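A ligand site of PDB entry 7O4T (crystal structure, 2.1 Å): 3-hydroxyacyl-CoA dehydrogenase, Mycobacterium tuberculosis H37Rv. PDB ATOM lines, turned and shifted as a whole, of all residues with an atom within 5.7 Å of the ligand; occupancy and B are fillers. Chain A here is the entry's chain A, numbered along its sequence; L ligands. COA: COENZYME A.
S1P of the ligand sits close to N of Gly 84, 3.0 Å away.
N6A of the ligand sits at hydrogen-bond distance from O of Gly 84.
An oxygen (O2B) of the ligand sits at hydrogen-bond distance from the side-chain amide oxygen (OE1) of Gln 324, 3.0 Å away.
N1A of the ligand is in hydrogen-bond range of N of Val 86 (3.2 Å).
S1P of the ligand sits close to N of Gly 132 (3.6 Å).
The side-chain carboxylate (OE2) of Glu 157 sits close to a sulfur (S1P) of the ligand, at 3.7 Å.
OG1 of Thr 79 lies within hydrogen-bond range of OG1 of Thr 43, 3.1 Å away.
NH1 of Arg 191 sits at hydrogen-bond distance from OE1 of Gln 152, at 3.4 Å.
N of Leu 162 lies within hydrogen-bond range of O of Glu 157, at 2.9 Å.
N of Lys 87 sits close to OD1 of Asp 85 (3.4 Å).
Ser 42 touches the ligand.
CG2 of Thr 43 touches O4B of the ligand, at 3.5 Å.
CG2 of Val 45 touches C6A of the ligand, at 3.6 Å.
O of Ala 82 touches C6P of the ligand (3.2 Å).
Gly 83 touches the ligand (CA to S1P, 3.7 Å).
CA of Asp 85 touches N1A of the ligand, at 3.7 Å.
Leu 130 touches the ligand.
CA of Gly 131 touches S1P of the ligand (3.8 Å).
Pro 156 touches the ligand (CG to O5P, 3.4 Å).
Leu 160 touches the ligand.
NH1 of Arg 191 touches O9P of the ligand, 3.5 Å away.
CZ of Phe 320 touches C4A of the ligand, 3.7 Å away.
Hydrophobic or aromatic side chains that line the ligand: Val 45, Ala 82, Val 86, Leu 130, Pro 156, Leu 160 and Phe 320.
Of the 23 residues printed, 17 come within 4 Å of the ligand.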
ATOM      1  N   SER A  42      14.179  23.902 -25.565  1.00  0.00           N
ATOM      2  CA  SER A  42      13.936  23.602 -24.162  1.00  0.00           C
ATOM      3  C   SER A  42      13.722  22.115 -23.895  1.00  0.00           C
ATOM      4  O   SER A  42      13.653  21.711 -22.736  1.00  0.00           O
ATOM      5  CB  SER A  42      12.721  24.383 -23.654  1.00  0.00           C
ATOM      6  OG  SER A  42      11.587  24.141 -24.471  1.00  0.00           O
ATOM      7  N   THR A  43      13.621  21.293 -24.943  1.00  0.00           N
ATOM      8  CA  THR A  43      13.372  19.866 -24.774  1.00  0.00           C
ATOM      9  C   THR A  43      14.202  19.091 -25.787  1.00  0.00           C
ATOM     10  O   THR A  43      14.591  19.605 -26.833  1.00  0.00           O
ATOM     11  CB  THR A  43      11.884  19.533 -24.929  1.00  0.00           C
ATOM     12  OG1 THR A  43      11.644  18.199 -24.495  1.00  0.00           O
ATOM     13  CG2 THR A  43      11.447  19.681 -26.389  1.00  0.00           C
ATOM     14  N   VAL A  45      14.668  16.326 -28.609  1.00  0.00           N
ATOM     15  CA  VAL A  45      13.815  15.895 -29.717  1.00  0.00           C
ATOM     16  C   VAL A  45      14.664  15.164 -30.744  1.00  0.00           C
ATOM     17  O   VAL A  45      15.801  15.564 -31.021  1.00  0.00           O
ATOM     18  CB  VAL A  45      13.075  17.107 -30.336  1.00  0.00           C
ATOM     19  CG1 VAL A  45      12.888  16.928 -31.832  1.00  0.00           C
ATOM     20  CG2 VAL A  45      11.738  17.318 -29.653  1.00  0.00           C
ATOM     21  N   THR A  79      12.272  17.856 -18.838  1.00  0.00           N
ATOM     22  CA  THR A  79      11.807  16.549 -19.271  1.00  0.00           C
ATOM     23  C   THR A  79      12.986  15.671 -19.662  1.00  0.00           C
ATOM     24  O   THR A  79      14.111  16.139 -19.875  1.00  0.00           O
ATOM     25  CB  THR A  79      10.845  16.684 -20.450  1.00  0.00           C
ATOM     26  OG1 THR A  79      11.481  17.395 -21.508  1.00  0.00           O
ATOM     27  CG2 THR A  79       9.586  17.431 -20.027  1.00  0.00           C
ATOM     28  N   ALA A  82      11.431  14.338 -25.444  1.00  0.00           N
ATOM     29  CA  ALA A  82      10.066  14.635 -25.861  1.00  0.00           C
ATOM     30  C   ALA A  82       9.587  13.754 -27.005  1.00  0.00           C
ATOM     31  O   ALA A  82       8.380  13.488 -27.122  1.00  0.00           O
ATOM     32  CB  ALA A  82       9.937  16.099 -26.254  1.00  0.00           C
ATOM     33  N   GLY A  83      10.482  13.306 -27.885  1.00  0.00           N
ATOM     34  CA  GLY A  83      10.127  12.403 -28.966  1.00  0.00           C
ATOM     35  C   GLY A  83      10.556  12.936 -30.317  1.00  0.00           C
ATOM     36  O   GLY A  83      11.540  13.674 -30.430  1.00  0.00           O
ATOM     37  N   GLY A  84       9.800  12.542 -31.345  1.00  0.00           N
ATOM     38  CA  GLY A  84      10.162  12.898 -32.711  1.00  0.00           C
ATOM     39  C   GLY A  84       9.865  14.349 -33.039  1.00  0.00           C
ATOM     40  O   GLY A  84       9.069  15.019 -32.388  1.00  0.00           O
ATOM     41  N   ASP A  85      10.518  14.814 -34.101  1.00  0.00           N
ATOM     42  CA  ASP A  85      10.383  16.194 -34.559  1.00  0.00           C
ATOM     43  C   ASP A  85       9.136  16.312 -35.422  1.00  0.00           C
ATOM     44  O   ASP A  85       9.140  15.916 -36.596  1.00  0.00           O
ATOM     45  CB  ASP A  85      11.633  16.626 -35.326  1.00  0.00           C
ATOM     46  CG  ASP A  85      11.619  18.102 -35.692  1.00  0.00           C
ATOM     47  OD1 ASP A  85      10.729  18.839 -35.209  1.00  0.00           O
ATOM     48  OD2 ASP A  85      12.485  18.526 -36.480  1.00  0.00           O
ATOM     49  N   VAL A  86       8.068  16.858 -34.852  1.00  0.00           N
ATOM     50  CA  VAL A  86       6.796  16.940 -35.561  1.00  0.00           C
ATOM     51  C   VAL A  86       6.885  17.934 -36.717  1.00  0.00           C
ATOM     52  O   VAL A  86       6.243  17.744 -37.762  1.00  0.00           O
ATOM     53  CB  VAL A  86       5.658  17.295 -34.596  1.00  0.00           C
ATOM     54  CG1 VAL A  86       4.326  17.368 -35.327  1.00  0.00           C
ATOM     55  CG2 VAL A  86       5.584  16.280 -33.471  1.00  0.00           C
ATOM     56  N   LYS A  87       7.668  19.002 -36.564  1.00  0.00           N
ATOM     57  CA  LYS A  87       7.787  19.995 -37.633  1.00  0.00           C
ATOM     58  C   LYS A  87       8.376  19.383 -38.897  1.00  0.00           C
ATOM     59  O   LYS A  87       8.057  19.819 -40.008  1.00  0.00           O
ATOM     60  CB  LYS A  87       8.622  21.184 -37.169  1.00  0.00           C
ATOM     61  CG  LYS A  87       8.618  22.357 -38.145  1.00  0.00           C
ATOM     62  CD  LYS A  87       9.621  23.425 -37.738  1.00  0.00           C
ATOM     63  CE  LYS A  87       9.694  24.536 -38.777  1.00  0.00           C
ATOM     64  NZ  LYS A  87      10.756  25.533 -38.457  1.00  0.00           N
ATOM     65  N   MET A  89       8.252  15.841 -39.526  1.00  0.00           N
ATOM     66  CA  MET A  89       7.434  14.705 -39.943  1.00  0.00           C
ATOM     67  C   MET A  89       6.180  15.150 -40.695  1.00  0.00           C
ATOM     68  O   MET A  89       5.682  14.419 -41.556  1.00  0.00           O
ATOM     69  CB  MET A  89       7.041  13.859 -38.736  1.00  0.00           C
ATOM     70  CG  MET A  89       8.199  13.090 -38.108  1.00  0.00           C
ATOM     71  SD  MET A  89       7.668  11.971 -36.809  1.00  0.00           S
ATOM     72  CE  MET A  89       6.954  13.104 -35.623  1.00  0.00           C
ATOM     73  N   ALA A 128       9.439  13.892 -18.266  1.00  0.00           N
ATOM     74  CA  ALA A 128       8.569  13.246 -19.246  1.00  0.00           C
ATOM     75  C   ALA A 128       9.402  12.509 -20.289  1.00  0.00           C
ATOM     76  O   ALA A 128      10.334  13.073 -20.871  1.00  0.00           O
ATOM     77  CB  ALA A 128       7.674  14.285 -19.919  1.00  0.00           C
ATOM     78  N   LEU A 130       8.358  10.590 -23.585  1.00  0.00           N
ATOM     79  CA  LEU A 130       7.208  10.358 -24.442  1.00  0.00           C
ATOM     80  C   LEU A 130       7.658  10.053 -25.859  1.00  0.00           C
ATOM     81  O   LEU A 130       8.548  10.726 -26.400  1.00  0.00           O
ATOM     82  CB  LEU A 130       6.263  11.562 -24.452  1.00  0.00           C
ATOM     83  CG  LEU A 130       5.582  11.860 -23.112  1.00  0.00           C
ATOM     84  CD1 LEU A 130       4.748  13.123 -23.202  1.00  0.00           C
ATOM     85  CD2 LEU A 130       4.728  10.680 -22.674  1.00  0.00           C
ATOM     86  N   GLY A 131       7.038   9.046 -26.462  1.00  0.00           N
ATOM     87  CA  GLY A 131       7.330   8.724 -27.848  1.00  0.00           C
ATOM     88  C   GLY A 131       8.746   8.232 -28.012  1.00  0.00           C
ATOM     89  O   GLY A 131       9.162   7.252 -27.377  1.00  0.00           O
ATOM     90  N   GLY A 132       9.513   8.912 -28.869  1.00  0.00           N
ATOM     91  CA  GLY A 132      10.910   8.560 -29.037  1.00  0.00           C
ATOM     92  C   GLY A 132      11.701   8.616 -27.741  1.00  0.00           C
ATOM     93  O   GLY A 132      12.708   7.928 -27.587  1.00  0.00           O
ATOM     94  N   GLN A 152       5.494  12.200 -17.152  1.00  0.00           N
ATOM     95  CA  GLN A 152       4.640  11.288 -17.907  1.00  0.00           C
ATOM     96  C   GLN A 152       5.505  10.350 -18.733  1.00  0.00           C
ATOM     97  O   GLN A 152       6.588  10.710 -19.188  1.00  0.00           O
ATOM     98  CB  GLN A 152       3.677  12.053 -18.840  1.00  0.00           C
ATOM     99  CG  GLN A 152       2.634  12.888 -18.118  1.00  0.00           C
ATOM    100  CD  GLN A 152       1.757  13.660 -19.080  1.00  0.00           C
ATOM    101  OE1 GLN A 152       2.233  14.193 -20.081  1.00  0.00           O
ATOM    102  NE2 GLN A 152       0.468  13.714 -18.782  1.00  0.00           N
ATOM    103  N   PRO A 156       2.592   8.071 -27.300  1.00  0.00           N
ATOM    104  CA  PRO A 156       1.357   8.669 -27.814  1.00  0.00           C
ATOM    105  C   PRO A 156       1.342   8.887 -29.322  1.00  0.00           C
ATOM    106  O   PRO A 156       0.594   9.741 -29.807  1.00  0.00           O
ATOM    107  CB  PRO A 156       1.291  10.000 -27.063  1.00  0.00           C
ATOM    108  CG  PRO A 156       2.724  10.381 -26.912  1.00  0.00           C
ATOM    109  CD  PRO A 156       3.497   9.094 -26.735  1.00  0.00           C
ATOM    110  N   GLU A 157       2.154   8.135 -30.067  1.00  0.00           N
ATOM    111  CA  GLU A 157       2.249   8.361 -31.504  1.00  0.00           C
ATOM    112  C   GLU A 157       0.908   8.165 -32.204  1.00  0.00           C
ATOM    113  O   GLU A 157       0.578   8.883 -33.150  1.00  0.00           O
ATOM    114  CB  GLU A 157       3.312   7.452 -32.119  1.00  0.00           C
ATOM    115  CG  GLU A 157       4.747   7.951 -31.953  1.00  0.00           C
ATOM    116  CD  GLU A 157       5.373   7.528 -30.640  1.00  0.00           C
ATOM    117  OE1 GLU A 157       4.642   7.378 -29.645  1.00  0.00           O
ATOM    118  OE2 GLU A 157       6.610   7.340 -30.614  1.00  0.00           O
ATOM    119  N   LEU A 160      -1.238  11.098 -32.829  1.00  0.00           N
ATOM    120  CA  LEU A 160      -0.895  11.976 -33.942  1.00  0.00           C
ATOM    121  C   LEU A 160      -0.970  11.254 -35.287  1.00  0.00           C
ATOM    122  O   LEU A 160      -0.389  11.721 -36.275  1.00  0.00           O
ATOM    123  CB  LEU A 160       0.490  12.571 -33.739  1.00  0.00           C
ATOM    124  CG  LEU A 160       0.752  13.268 -32.402  1.00  0.00           C
ATOM    125  CD1 LEU A 160       2.179  13.780 -32.344  1.00  0.00           C
ATOM    126  CD2 LEU A 160      -0.228  14.395 -32.160  1.00  0.00           C
ATOM    127  N   LEU A 162       0.416   8.413 -36.000  1.00  0.00           N
ATOM    128  CA  LEU A 162       1.695   7.751 -36.224  1.00  0.00           C
ATOM    129  C   LEU A 162       1.743   6.463 -35.407  1.00  0.00           C
ATOM    130  O   LEU A 162       0.749   6.055 -34.788  1.00  0.00           O
ATOM    131  CB  LEU A 162       2.852   8.686 -35.856  1.00  0.00           C
ATOM    132  CG  LEU A 162       2.835  10.066 -36.531  1.00  0.00           C
ATOM    133  CD1 LEU A 162       3.923  10.950 -35.959  1.00  0.00           C
ATOM    134  CD2 LEU A 162       2.988   9.923 -38.022  1.00  0.00           C
ATOM    135  N   ARG A 191      -0.754   7.910 -21.588  1.00  0.00           N
ATOM    136  CA  ARG A 191       0.319   8.556 -20.831  1.00  0.00           C
ATOM    137  C   ARG A 191       0.195   8.138 -19.374  1.00  0.00           C
ATOM    138  O   ARG A 191      -0.855   8.321 -18.751  1.00  0.00           O
ATOM    139  CB  ARG A 191       0.237  10.080 -20.962  1.00  0.00           C
ATOM    140  CG  ARG A 191       0.183  10.559 -22.399  1.00  0.00           C
ATOM    141  CD  ARG A 191       0.532  12.031 -22.502  1.00  0.00           C
ATOM    142  NE  ARG A 191       0.488  12.511 -23.878  1.00  0.00           N
ATOM    143  CZ  ARG A 191       0.934  13.695 -24.277  1.00  0.00           C
ATOM    144  NH1 ARG A 191       1.458  14.540 -23.396  1.00  0.00           N
ATOM    145  NH2 ARG A 191       0.855  14.045 -25.550  1.00  0.00           N
ATOM    146  N   PHE A 320      -1.203  18.555 -32.293  1.00  0.00           N
ATOM    147  CA  PHE A 320       0.061  19.148 -31.882  1.00  0.00           C
ATOM    148  C   PHE A 320       0.077  20.652 -32.114  1.00  0.00           C
ATOM    149  O   PHE A 320       0.165  21.408 -31.143  1.00  0.00           O
ATOM    150  CB  PHE A 320       1.245  18.487 -32.590  1.00  0.00           C
ATOM    151  CG  PHE A 320       2.581  18.946 -32.085  1.00  0.00           C
ATOM    152  CD1 PHE A 320       3.133  18.398 -30.935  1.00  0.00           C
ATOM    153  CD2 PHE A 320       3.287  19.940 -32.746  1.00  0.00           C
ATOM    154  CE1 PHE A 320       4.356  18.822 -30.463  1.00  0.00           C
ATOM    155  CE2 PHE A 320       4.519  20.367 -32.278  1.00  0.00           C
ATOM    156  CZ  PHE A 320       5.049  19.813 -31.130  1.00  0.00           C
ATOM    157  N   GLN A 324      -1.338  23.446 -29.489  1.00  0.00           N
ATOM    158  CA  GLN A 324      -0.269  24.226 -28.878  1.00  0.00           C
ATOM    159  C   GLN A 324      -0.536  25.720 -29.031  1.00  0.00           C
ATOM    160  O   GLN A 324      -0.249  26.509 -28.118  1.00  0.00           O
ATOM    161  CB  GLN A 324       1.069  23.846 -29.503  1.00  0.00           C
ATOM    162  CG  GLN A 324       2.285  24.207 -28.661  1.00  0.00           C
ATOM    163  CD  GLN A 324       3.412  23.211 -28.839  1.00  0.00           C
ATOM    164  OE1 GLN A 324       4.454  23.535 -29.401  1.00  0.00           O
ATOM    165  NE2 GLN A 324       3.201  21.997 -28.344  1.00  0.00           N
HETATM  166  N1A COA L   1       8.570  17.770 -31.787  1.00  0.00           N
HETATM  167  C2A COA L   1       8.906  19.049 -31.982  1.00  0.00           C
HETATM  168  N3A COA L   1       8.947  20.059 -31.117  1.00  0.00           N
HETATM  169  C4A COA L   1       8.576  19.648 -29.897  1.00  0.00           C
HETATM  170  C5A COA L   1       8.202  18.373 -29.531  1.00  0.00           C
HETATM  171  C6A COA L   1       8.203  17.385 -30.541  1.00  0.00           C
HETATM  172  N6A COA L   1       7.870  16.120 -30.330  1.00  0.00           N
HETATM  173  N7A COA L   1       7.890  18.330 -28.175  1.00  0.00           N
HETATM  174  C8A COA L   1       8.085  19.556 -27.758  1.00  0.00           C
HETATM  175  N9A COA L   1       8.496  20.405 -28.757  1.00  0.00           N
HETATM  176  C1B COA L   1       8.801  21.823 -28.652  1.00  0.00           C
HETATM  177  C2B COA L   1       7.635  22.755 -28.930  1.00  0.00           C
HETATM  178  O2B COA L   1       7.293  22.867 -30.293  1.00  0.00           O
HETATM  179  C3B COA L   1       8.150  24.052 -28.296  1.00  0.00           C
HETATM  180  O3B COA L   1       9.082  24.677 -29.180  1.00  0.00           O
HETATM  181  P3B COA L   1       8.984  26.278 -29.035  1.00  0.00           P
HETATM  182  O7A COA L   1       7.706  26.690 -29.751  1.00  0.00           O
HETATM  183  O8A COA L   1       8.926  26.609 -27.562  1.00  0.00           O
HETATM  184  O9A COA L   1      10.217  26.855 -29.701  1.00  0.00           O
HETATM  185  C4B COA L   1       8.909  23.527 -27.065  1.00  0.00           C
HETATM  186  O4B COA L   1       9.156  22.116 -27.319  1.00  0.00           O
HETATM  187  C5B COA L   1       8.182  23.672 -25.762  1.00  0.00           C
HETATM  188  O5B COA L   1       6.933  22.924 -25.823  1.00  0.00           O
HETATM  189  P1A COA L   1       5.828  23.145 -24.689  1.00  0.00           P
HETATM  190  O1A COA L   1       4.646  22.279 -24.968  1.00  0.00           O
HETATM  191  O2A COA L   1       5.604  24.606 -24.496  1.00  0.00           O
HETATM  192  O3A COA L   1       6.589  22.568 -23.393  1.00  0.00           O
HETATM  193  P2A COA L   1       6.086  21.570 -22.248  1.00  0.00           P
HETATM  194  O4A COA L   1       7.132  21.471 -21.178  1.00  0.00           O
HETATM  195  O5A COA L   1       4.683  21.910 -21.861  1.00  0.00           O
HETATM  196  O6A COA L   1       6.066  20.187 -23.057  1.00  0.00           O
HETATM  197  CBP COA L   1       5.547  17.860 -23.450  1.00  0.00           C
HETATM  198  CCP COA L   1       5.609  18.975 -22.402  1.00  0.00           C
HETATM  199  CDP COA L   1       6.966  17.470 -23.852  1.00  0.00           C
HETATM  200  CEP COA L   1       4.849  16.641 -22.838  1.00  0.00           C
HETATM  201  CAP COA L   1       4.774  18.350 -24.680  1.00  0.00           C
HETATM  202  OAP COA L   1       5.582  19.246 -25.415  1.00  0.00           O
HETATM  203  C9P COA L   1       4.252  17.241 -25.589  1.00  0.00           C
HETATM  204  O9P COA L   1       3.095  16.854 -25.480  1.00  0.00           O
HETATM  205  N8P COA L   1       5.089  16.764 -26.499  1.00  0.00           N
HETATM  206  C7P COA L   1       4.644  15.879 -27.577  1.00  0.00           C
HETATM  207  C6P COA L   1       5.342  14.530 -27.556  1.00  0.00           C
HETATM  208  C5P COA L   1       4.713  13.579 -28.552  1.00  0.00           C
HETATM  209  O5P COA L   1       3.532  13.247 -28.449  1.00  0.00           O
HETATM  210  N4P COA L   1       5.493  13.127 -29.546  1.00  0.00           N
HETATM  211  C3P COA L   1       4.992  12.271 -30.614  1.00  0.00           C
HETATM  212  C2P COA L   1       6.049  11.950 -31.636  1.00  0.00           C
HETATM  213  S1P COA L   1       7.373  10.893 -30.984  1.00  0.00           S
